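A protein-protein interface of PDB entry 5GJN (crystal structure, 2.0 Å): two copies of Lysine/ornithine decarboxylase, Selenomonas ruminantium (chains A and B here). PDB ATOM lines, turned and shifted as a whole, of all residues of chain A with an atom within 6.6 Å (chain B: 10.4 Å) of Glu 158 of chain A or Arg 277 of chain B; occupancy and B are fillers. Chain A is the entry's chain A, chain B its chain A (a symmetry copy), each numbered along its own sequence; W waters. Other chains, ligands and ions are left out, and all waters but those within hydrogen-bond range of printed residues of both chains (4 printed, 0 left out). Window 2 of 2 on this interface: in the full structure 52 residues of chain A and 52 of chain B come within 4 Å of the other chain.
The side-chain carboxylate (OD2) of Asp 116 of chain A is in salt-bridge range of the side-chain amino group (NZ) of Lys 275 of chain B (3.5 Å).
The guanidinium group of Arg 277 of chain B is in hydrogen-bond range of the backbone carbonyl oxygen of Asp 116 of chain A (2.9 Å).
The side-chain carboxylate (OD1) of Asp 117 of chain A is in salt-bridge range of the guanidinium group (NH2) of Arg 277 of chain B, 3.96 Å away.
OE1 of Glu 158 of chain A lies within salt-bridge range of NH2 of Arg 277 of chain B (2.8 Å).
The side-chain carboxylate (OD2) of Asp 117 of chain A sits close to the backbone carbonyl oxygen (O) of Thr 274 of chain B, at 2.9 Å.
The side-chain carboxylate (OD2) of Asp 116 of chain A lies within hydrogen-bond range of the backbone NH (N) of Gly 153 of chain A (2.9 Å).
The backbone carbonyl oxygen (O) of Trp 282 of chain B is in hydrogen-bond range of the backbone NH (N) of Lys 275 of chain B, 2.9 Å away.
Asp 117 of chain A touches Lys 275 of chain B.
Arg 277 of chain B touches Ala 154 of chain A (NH2 to CB, 3.8 Å).
Pro 155 of chain A touches Arg 277 of chain B.
Of chain B, only Arg 277 comes within 4 Å of Glu 158 of chain A.
Asp 117 of chain A touches just these residues of chain B: Thr 274 (2.9 Å), Lys 275 (3.4 Å) and Arg 277 (3.96 Å).
Of chain B, only Arg 277 (3.8 Å) comes within 4 Å of Ala 154 of chain A.
Pro 155 of chain A touches just one residue of chain B: Arg 277.
No residue of chain B comes within 4 Å of Ala 159 of chain A.
No residue of chain B comes within 4 Å of Asp 161 of chain A.
Of the printed residues of chain A, Lys 275 of chain B touches Asp 116 and Asp 117.
Of the printed residues of chain A, Thr 274 of chain B touches Asp 117.
Printed residues of chain B within 4 Å of Asp 116 of chain A: Lys 275 and Arg 277.
Thr 276 of chain B touches none of the printed residues of chain A.
Glu 157 of chain A touches none of the printed residues of chain B.
The nearest printed residue of chain A that does not touch Arg 277 of chain B is Pro 118 of chain A (4.02 Å).
Printed residues of chain B that touch a printed residue of chain A: Thr 274, Lys 275 and Arg 277.
Of the 15 printed residues of chain A, 5 touch a printed residue of chain B.
Printed residues of chain A that touch a printed residue of chain B: Asp 116, Asp 117, Ala 154, Pro 155 and Glu 158.
Among the printed residues, 8 pairs touch across the chains.
Among the printed residues, Asp or Glu carboxylates within 4 Å of a Lys or Arg side-chain nitrogen of the other chain: Asp 116 of chain A with Lys 275 of chain B, Asp 117 of chain A with Arg 277 of chain B and Glu 158 of chain A with Arg 277 of chain B.
No position is printed for both chains.
Water W1 lies within hydrogen-bond range of OD1 of Asp 117 of chain A (2.6 Å), N of Thr 276 of chain B (3.0 Å) and N of Arg 277 of chain B (3.1 Å).
Water W2 bridges the side-chain carboxylate (OD1) of Asp 116 of chain A and the side-chain amino group (NZ) of Lys 275 of chain B.
Water W3 lies within hydrogen-bond range of OD2 of Asp 117 of chain A (2.7 Å), N of Thr 276 of chain B (3.0 Å) and OG1 of Thr 274 of chain B (3.0 Å).
Water W4 bridges NZ of Lys 275 of chain B (2.8 Å) and O of Gly 153 of chain A (3.2 Å).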
ATOM      1  N   ASP A 116     -10.124 -20.603  18.184  1.00  0.00           N
ATOM      2  CA  ASP A 116      -9.856 -21.293  19.432  1.00  0.00           C
ATOM      3  C   ASP A 116      -8.728 -22.326  19.416  1.00  0.00           C
ATOM      4  O   ASP A 116      -8.549 -23.024  20.380  1.00  0.00           O
ATOM      5  CB  ASP A 116     -11.128 -21.921  19.979  1.00  0.00           C
ATOM      6  CG  ASP A 116     -11.615 -23.072  19.144  1.00  0.00           C
ATOM      7  OD1 ASP A 116     -10.858 -23.582  18.323  1.00  0.00           O
ATOM      8  OD2 ASP A 116     -12.764 -23.472  19.316  1.00  0.00           O
ATOM      9  N   ASP A 117      -8.004 -22.447  18.317  1.00  0.00           N
ATOM     10  CA  ASP A 117      -7.032 -23.516  18.183  1.00  0.00           C
ATOM     11  C   ASP A 117      -5.757 -23.087  17.484  1.00  0.00           C
ATOM     12  O   ASP A 117      -5.816 -22.289  16.580  1.00  0.00           O
ATOM     13  CB  ASP A 117      -7.674 -24.654  17.409  1.00  0.00           C
ATOM     14  CG  ASP A 117      -6.948 -25.944  17.585  1.00  0.00           C
ATOM     15  OD1 ASP A 117      -7.236 -26.655  18.541  1.00  0.00           O
ATOM     16  OD2 ASP A 117      -6.082 -26.239  16.763  1.00  0.00           O
ATOM     17  N   PRO A 118      -4.633 -23.685  17.816  1.00  0.00           N
ATOM     18  CA  PRO A 118      -3.396 -23.313  17.146  1.00  0.00           C
ATOM     19  C   PRO A 118      -3.512 -23.565  15.647  1.00  0.00           C
ATOM     20  O   PRO A 118      -2.974 -22.805  14.882  1.00  0.00           O
ATOM     21  CB  PRO A 118      -2.368 -24.234  17.782  1.00  0.00           C
ATOM     22  CG  PRO A 118      -2.912 -24.514  19.120  1.00  0.00           C
ATOM     23  CD  PRO A 118      -4.392 -24.582  18.950  1.00  0.00           C
ATOM     24  N   VAL A 135      -9.791 -14.476  20.590  1.00  0.00           N
ATOM     25  CA  VAL A 135      -9.748 -15.860  20.984  1.00  0.00           C
ATOM     26  C   VAL A 135     -11.012 -16.194  21.726  1.00  0.00           C
ATOM     27  O   VAL A 135     -11.438 -15.495  22.664  1.00  0.00           O
ATOM     28  CB  VAL A 135      -8.434 -16.212  21.808  1.00  0.00           C
ATOM     29  CG1 VAL A 135      -8.271 -15.464  23.134  1.00  0.00           C
ATOM     30  CG2 VAL A 135      -8.311 -17.705  22.043  1.00  0.00           C
ATOM     31  N   GLY A 153     -13.966 -23.192  21.910  1.00  0.00           N
ATOM     32  CA  GLY A 153     -13.375 -22.546  23.057  1.00  0.00           C
ATOM     33  C   GLY A 153     -12.111 -23.186  23.570  1.00  0.00           C
ATOM     34  O   GLY A 153     -12.058 -24.368  23.824  1.00  0.00           O
ATOM     35  N   ALA A 154     -11.092 -22.367  23.747  1.00  0.00           N
ATOM     36  CA  ALA A 154      -9.834 -22.813  24.274  1.00  0.00           C
ATOM     37  C   ALA A 154      -9.890 -22.719  25.776  1.00  0.00           C
ATOM     38  O   ALA A 154     -10.662 -21.956  26.329  1.00  0.00           O
ATOM     39  CB  ALA A 154      -8.718 -21.953  23.747  1.00  0.00           C
ATOM     40  N   PRO A 155      -9.062 -23.511  26.431  1.00  0.00           N
ATOM     41  CA  PRO A 155      -8.939 -23.405  27.865  1.00  0.00           C
ATOM     42  C   PRO A 155      -8.489 -22.017  28.191  1.00  0.00           C
ATOM     43  O   PRO A 155      -7.643 -21.442  27.495  1.00  0.00           O
ATOM     44  CB  PRO A 155      -7.821 -24.454  28.200  1.00  0.00           C
ATOM     45  CG  PRO A 155      -8.102 -25.516  27.162  1.00  0.00           C
ATOM     46  CD  PRO A 155      -8.281 -24.661  25.921  1.00  0.00           C
ATOM     47  N   VAL A 156      -9.065 -21.489  29.262  1.00  0.00           N
ATOM     48  CA  VAL A 156      -8.794 -20.167  29.723  1.00  0.00           C
ATOM     49  C   VAL A 156      -7.336 -19.956  29.801  1.00  0.00           C
ATOM     50  O   VAL A 156      -6.821 -18.967  29.299  1.00  0.00           O
ATOM     51  CB  VAL A 156      -9.445 -19.949  31.098  1.00  0.00           C
ATOM     52  CG1 VAL A 156      -8.899 -18.688  31.732  1.00  0.00           C
ATOM     53  CG2 VAL A 156     -10.928 -19.903  30.958  1.00  0.00           C
ATOM     54  N   GLU A 157      -6.619 -20.910  30.409  1.00  0.00           N
ATOM     55  CA  GLU A 157      -5.198 -20.716  30.604  1.00  0.00           C
ATOM     56  C   GLU A 157      -4.324 -20.950  29.334  1.00  0.00           C
ATOM     57  O   GLU A 157      -3.135 -20.720  29.351  1.00  0.00           O
ATOM     58  CB  GLU A 157      -4.705 -21.499  31.839  1.00  0.00           C
ATOM     59  CG  GLU A 157      -5.377 -21.097  33.203  1.00  0.00           C
ATOM     60  CD  GLU A 157      -5.436 -19.569  33.473  1.00  0.00           C
ATOM     61  OE1 GLU A 157      -4.466 -18.812  33.151  1.00  0.00           O
ATOM     62  OE2 GLU A 157      -6.486 -19.101  34.001  1.00  0.00           O
ATOM     63  N   GLU A 158      -4.950 -21.326  28.235  1.00  0.00           N
ATOM     64  CA  GLU A 158      -4.291 -21.322  26.940  1.00  0.00           C
ATOM     65  C   GLU A 158      -4.522 -20.039  26.109  1.00  0.00           C
ATOM     66  O   GLU A 158      -3.881 -19.844  25.099  1.00  0.00           O
ATOM     67  CB  GLU A 158      -4.764 -22.540  26.166  1.00  0.00           C
ATOM     68  CG  GLU A 158      -3.886 -22.971  25.018  1.00  0.00           C
ATOM     69  CD  GLU A 158      -4.398 -24.226  24.346  1.00  0.00           C
ATOM     70  OE1 GLU A 158      -4.441 -24.246  23.107  1.00  0.00           O
ATOM     71  OE2 GLU A 158      -4.755 -25.182  25.054  1.00  0.00           O
ATOM     72  N   ALA A 159      -5.427 -19.171  26.555  1.00  0.00           N
ATOM     73  CA  ALA A 159      -5.944 -18.074  25.741  1.00  0.00           C
ATOM     74  C   ALA A 159      -4.921 -17.079  25.295  1.00  0.00           C
ATOM     75  O   ALA A 159      -4.829 -16.761  24.105  1.00  0.00           O
ATOM     76  CB  ALA A 159      -7.152 -17.392  26.415  1.00  0.00           C
ATOM     77  N   LEU A 160      -4.113 -16.585  26.217  1.00  0.00           N
ATOM     78  CA  LEU A 160      -3.116 -15.605  25.879  1.00  0.00           C
ATOM     79  C   LEU A 160      -1.944 -16.192  25.026  1.00  0.00           C
ATOM     80  O   LEU A 160      -1.409 -15.482  24.204  1.00  0.00           O
ATOM     81  CB  LEU A 160      -2.610 -14.901  27.148  1.00  0.00           C
ATOM     82  CG  LEU A 160      -3.709 -14.195  27.991  1.00  0.00           C
ATOM     83  CD1 LEU A 160      -3.204 -13.574  29.287  1.00  0.00           C
ATOM     84  CD2 LEU A 160      -4.385 -13.103  27.185  1.00  0.00           C
ATOM     85  N   ASP A 161      -1.548 -17.446  25.236  1.00  0.00           N
ATOM     86  CA  ASP A 161      -0.531 -18.085  24.317  1.00  0.00           C
ATOM     87  C   ASP A 161      -1.081 -18.178  22.902  1.00  0.00           C
ATOM     88  O   ASP A 161      -0.349 -17.965  21.926  1.00  0.00           O
ATOM     89  CB  ASP A 161      -0.159 -19.499  24.775  1.00  0.00           C
ATOM     90  CG  ASP A 161       0.415 -19.528  26.204  1.00  0.00           C
ATOM     91  OD1 ASP A 161       1.118 -18.546  26.546  1.00  0.00           O
ATOM     92  OD2 ASP A 161       0.084 -20.471  26.959  1.00  0.00           O
ATOM     93  N   LEU A 162      -2.395 -18.414  22.779  1.00  0.00           N
ATOM     94  CA  LEU A 162      -2.970 -18.458  21.424  1.00  0.00           C
ATOM     95  C   LEU A 162      -2.915 -17.107  20.784  1.00  0.00           C
ATOM     96  O   LEU A 162      -2.504 -17.031  19.643  1.00  0.00           O
ATOM     97  CB  LEU A 162      -4.409 -18.996  21.394  1.00  0.00           C
ATOM     98  CG  LEU A 162      -4.447 -20.493  21.507  1.00  0.00           C
ATOM     99  CD1 LEU A 162      -5.810 -20.918  21.998  1.00  0.00           C
ATOM    100  CD2 LEU A 162      -4.145 -21.049  20.132  1.00  0.00           C
ATOM    101  N   LEU A 163      -3.353 -16.064  21.498  1.00  0.00           N
ATOM    102  CA  LEU A 163      -3.282 -14.671  21.000  1.00  0.00           C
ATOM    103  C   LEU A 163      -1.823 -14.278  20.671  1.00  0.00           C
ATOM    104  O   LEU A 163      -1.596 -13.567  19.747  1.00  0.00           O
ATOM    105  CB  LEU A 163      -3.841 -13.645  22.026  1.00  0.00           C
ATOM    106  CG  LEU A 163      -5.391 -13.658  22.176  1.00  0.00           C
ATOM    107  CD1 LEU A 163      -5.915 -12.865  23.361  1.00  0.00           C
ATOM    108  CD2 LEU A 163      -6.032 -13.273  20.874  1.00  0.00           C
ATOM    109  N   GLY B 273     -10.081 -28.305  10.094  1.00  0.00           N
ATOM    110  CA  GLY B 273      -9.498 -27.915  11.349  1.00  0.00           C
ATOM    111  C   GLY B 273      -9.165 -29.158  12.114  1.00  0.00           C
ATOM    112  O   GLY B 273      -9.712 -30.207  11.848  1.00  0.00           O
ATOM    113  N   THR B 274      -8.266 -29.037  13.072  1.00  0.00           N
ATOM    114  CA  THR B 274      -8.057 -30.080  14.071  1.00  0.00           C
ATOM    115  C   THR B 274      -8.081 -29.471  15.441  1.00  0.00           C
ATOM    116  O   THR B 274      -7.834 -28.278  15.575  1.00  0.00           O
ATOM    117  CB  THR B 274      -6.643 -30.680  13.857  1.00  0.00           C
ATOM    118  OG1 THR B 274      -5.638 -29.655  14.032  1.00  0.00           O
ATOM    119  CG2 THR B 274      -6.513 -31.165  12.439  1.00  0.00           C
ATOM    120  N   LYS B 275      -8.356 -30.266  16.452  1.00  0.00           N
ATOM    121  CA  LYS B 275      -8.046 -29.911  17.814  1.00  0.00           C
ATOM    122  C   LYS B 275      -7.259 -31.086  18.375  1.00  0.00           C
ATOM    123  O   LYS B 275      -7.788 -32.186  18.442  1.00  0.00           O
ATOM    124  CB  LYS B 275      -9.281 -29.749  18.681  1.00  0.00           C
ATOM    125  CG  LYS B 275     -10.326 -28.769  18.146  1.00  0.00           C
ATOM    126  CD  LYS B 275     -11.660 -29.198  18.719  1.00  0.00           C
ATOM    127  CE  LYS B 275     -12.674 -28.108  18.722  1.00  0.00           C
ATOM    128  NZ  LYS B 275     -12.332 -26.976  19.645  1.00  0.00           N
ATOM    129  N   THR B 276      -6.015 -30.846  18.762  1.00  0.00           N
ATOM    130  CA  THR B 276      -5.151 -31.909  19.289  1.00  0.00           C
ATOM    131  C   THR B 276      -4.904 -31.837  20.793  1.00  0.00           C
ATOM    132  O   THR B 276      -4.162 -32.640  21.322  1.00  0.00           O
ATOM    133  CB  THR B 276      -3.801 -31.859  18.558  1.00  0.00           C
ATOM    134  OG1 THR B 276      -3.247 -30.536  18.678  1.00  0.00           O
ATOM    135  CG2 THR B 276      -3.989 -32.189  17.072  1.00  0.00           C
ATOM    136  N   ARG B 277      -5.505 -30.901  21.505  1.00  0.00           N
ATOM    137  CA  ARG B 277      -5.210 -30.798  22.938  1.00  0.00           C
ATOM    138  C   ARG B 277      -5.824 -31.902  23.803  1.00  0.00           C
ATOM    139  O   ARG B 277      -5.354 -32.093  24.914  1.00  0.00           O
ATOM    140  CB  ARG B 277      -5.577 -29.397  23.528  1.00  0.00           C
ATOM    141  CG  ARG B 277      -7.073 -29.113  23.645  1.00  0.00           C
ATOM    142  CD  ARG B 277      -7.330 -27.777  24.333  1.00  0.00           C
ATOM    143  NE  ARG B 277      -6.834 -26.595  23.577  1.00  0.00           N
ATOM    144  CZ  ARG B 277      -7.501 -25.922  22.626  1.00  0.00           C
ATOM    145  NH1 ARG B 277      -8.710 -26.313  22.249  1.00  0.00           N
ATOM    146  NH2 ARG B 277      -6.946 -24.834  22.044  1.00  0.00           N
ATOM    147  N   GLY B 278      -6.902 -32.555  23.372  1.00  0.00           N
ATOM    148  CA  GLY B 278      -7.594 -33.586  24.194  1.00  0.00           C
ATOM    149  C   GLY B 278      -6.844 -34.898  23.997  1.00  0.00           C
ATOM    150  O   GLY B 278      -5.991 -34.990  23.093  1.00  0.00           O
ATOM    151  N   GLU B 279      -7.137 -35.918  24.814  1.00  0.00           N
ATOM    152  CA  GLU B 279      -6.587 -37.280  24.573  1.00  0.00           C
ATOM    153  C   GLU B 279      -6.996 -37.746  23.184  1.00  0.00           C
ATOM    154  O   GLU B 279      -6.181 -38.248  22.407  1.00  0.00           O
ATOM    155  CB  GLU B 279      -7.062 -38.294  25.628  1.00  0.00           C
ATOM    156  CG  GLU B 279      -8.545 -38.686  25.565  1.00  0.00           C
ATOM    157  CD  GLU B 279      -8.910 -39.792  26.527  1.00  0.00           C
ATOM    158  OE1 GLU B 279      -7.992 -40.469  27.037  1.00  0.00           O
ATOM    159  OE2 GLU B 279     -10.119 -39.988  26.762  1.00  0.00           O
ATOM    160  N   GLN B 280      -8.254 -37.469  22.872  1.00  0.00           N
ATOM    161  CA  GLN B 280      -8.842 -37.805  21.598  1.00  0.00           C
ATOM    162  C   GLN B 280      -8.747 -36.617  20.657  1.00  0.00           C
ATOM    163  O   GLN B 280      -9.287 -35.552  20.935  1.00  0.00           O
ATOM    164  CB  GLN B 280     -10.302 -38.165  21.816  1.00  0.00           C
ATOM    165  CG  GLN B 280     -11.022 -38.667  20.588  1.00  0.00           C
ATOM    166  CD  GLN B 280     -12.159 -39.586  20.942  1.00  0.00           C
ATOM    167  OE1 GLN B 280     -12.059 -40.370  21.873  1.00  0.00           O
ATOM    168  NE2 GLN B 280     -13.246 -39.490  20.205  1.00  0.00           N
ATOM    169  N   PRO B 281      -8.048 -36.772  19.549  1.00  0.00           N
ATOM    170  CA  PRO B 281      -7.970 -35.690  18.573  1.00  0.00           C
ATOM    171  C   PRO B 281      -9.335 -35.464  17.928  1.00  0.00           C
ATOM    172  O   PRO B 281     -10.115 -36.393  17.827  1.00  0.00           O
ATOM    173  CB  PRO B 281      -6.971 -36.208  17.539  1.00  0.00           C
ATOM    174  CG  PRO B 281      -6.444 -37.487  18.073  1.00  0.00           C
ATOM    175  CD  PRO B 281      -7.445 -38.005  19.039  1.00  0.00           C
ATOM    176  N   TRP B 282      -9.593 -34.229  17.519  1.00  0.00           N
ATOM    177  CA  TRP B 282     -10.815 -33.850  16.834  1.00  0.00           C
ATOM    178  C   TRP B 282     -10.465 -33.367  15.449  1.00  0.00           C
ATOM    179  O   TRP B 282      -9.534 -32.607  15.271  1.00  0.00           O
ATOM    180  CB  TRP B 282     -11.496 -32.705  17.555  1.00  0.00           C
ATOM    181  CG  TRP B 282     -12.442 -33.092  18.589  1.00  0.00           C
ATOM    182  CD1 TRP B 282     -12.177 -33.800  19.706  1.00  0.00           C
ATOM    183  CD2 TRP B 282     -13.825 -32.764  18.639  1.00  0.00           C
ATOM    184  NE1 TRP B 282     -13.310 -33.951  20.451  1.00  0.00           N
ATOM    185  CE2 TRP B 282     -14.340 -33.317  19.816  1.00  0.00           C
ATOM    186  CE3 TRP B 282     -14.683 -32.060  17.796  1.00  0.00           C
ATOM    187  CZ2 TRP B 282     -15.671 -33.192  20.174  1.00  0.00           C
ATOM    188  CZ3 TRP B 282     -16.000 -31.935  18.157  1.00  0.00           C
ATOM    189  CH2 TRP B 282     -16.483 -32.499  19.330  1.00  0.00           C
ATOM    190  N   TYR B 283     -11.216 -33.820  14.464  1.00  0.00           N
ATOM    191  CA  TYR B 283     -11.056 -33.333  13.113  1.00  0.00           C
ATOM    192  C   TYR B 283     -12.328 -32.637  12.676  1.00  0.00           C
ATOM    193  O   TYR B 283     -13.402 -33.187  12.808  1.00  0.00           O
ATOM    194  CB  TYR B 283     -10.719 -34.483  12.178  1.00  0.00           C
ATOM    195  CG  TYR B 283      -9.470 -35.205  12.593  1.00  0.00           C
ATOM    196  CD1 TYR B 283      -8.229 -34.628  12.415  1.00  0.00           C
ATOM    197  CD2 TYR B 283      -9.530 -36.443  13.195  1.00  0.00           C
ATOM    198  CE1 TYR B 283      -7.080 -35.276  12.802  1.00  0.00           C
ATOM    199  CE2 TYR B 283      -8.384 -37.100  13.589  1.00  0.00           C
ATOM    200  CZ  TYR B 283      -7.163 -36.508  13.391  1.00  0.00           C
ATOM    201  OH  TYR B 283      -6.023 -37.148  13.778  1.00  0.00           O
ATOM    202  N   ILE B 284     -12.200 -31.431  12.146  1.00  0.00           N
ATOM    203  CA  ILE B 284     -13.350 -30.727  11.622  1.00  0.00           C
ATOM    204  C   ILE B 284     -13.386 -30.901  10.124  1.00  0.00           C
ATOM    205  O   ILE B 284     -12.464 -30.526   9.439  1.00  0.00           O
ATOM    206  CB  ILE B 284     -13.294 -29.220  11.915  1.00  0.00           C
ATOM    207  CG1 ILE B 284     -13.024 -28.963  13.387  1.00  0.00           C
ATOM    208  CG2 ILE B 284     -14.585 -28.546  11.487  1.00  0.00           C
ATOM    209  CD1 ILE B 284     -13.894 -29.764  14.306  1.00  0.00           C
ATOM    210  N   LYS B 314      -5.625 -43.755  16.515  1.00  0.00           N
ATOM    211  CA  LYS B 314      -6.160 -43.640  17.861  1.00  0.00           C
ATOM    212  C   LYS B 314      -7.633 -43.176  17.840  1.00  0.00           C
ATOM    213  O   LYS B 314      -8.079 -42.531  16.898  1.00  0.00           O
ATOM    214  CB  LYS B 314      -5.275 -42.716  18.703  1.00  0.00           C
ATOM    215  CG  LYS B 314      -4.471 -41.667  17.933  1.00  0.00           C
ATOM    216  CD  LYS B 314      -4.086 -40.456  18.776  1.00  0.00           C
ATOM    217  CE  LYS B 314      -3.217 -40.809  19.974  1.00  0.00           C
ATOM    218  NZ  LYS B 314      -2.788 -39.594  20.738  1.00  0.00           N
HETATM  219  O   HOH W   1      -5.882 -28.169  20.106  1.00  0.00           O
HETATM  220  O   HOH W   2     -11.646 -25.617  16.938  1.00  0.00           O
HETATM  221  O   HOH W   3      -5.096 -28.752  16.870  1.00  0.00           O
HETATM  222  O   HOH W   4     -13.066 -26.986  22.355  1.00  0.00           O
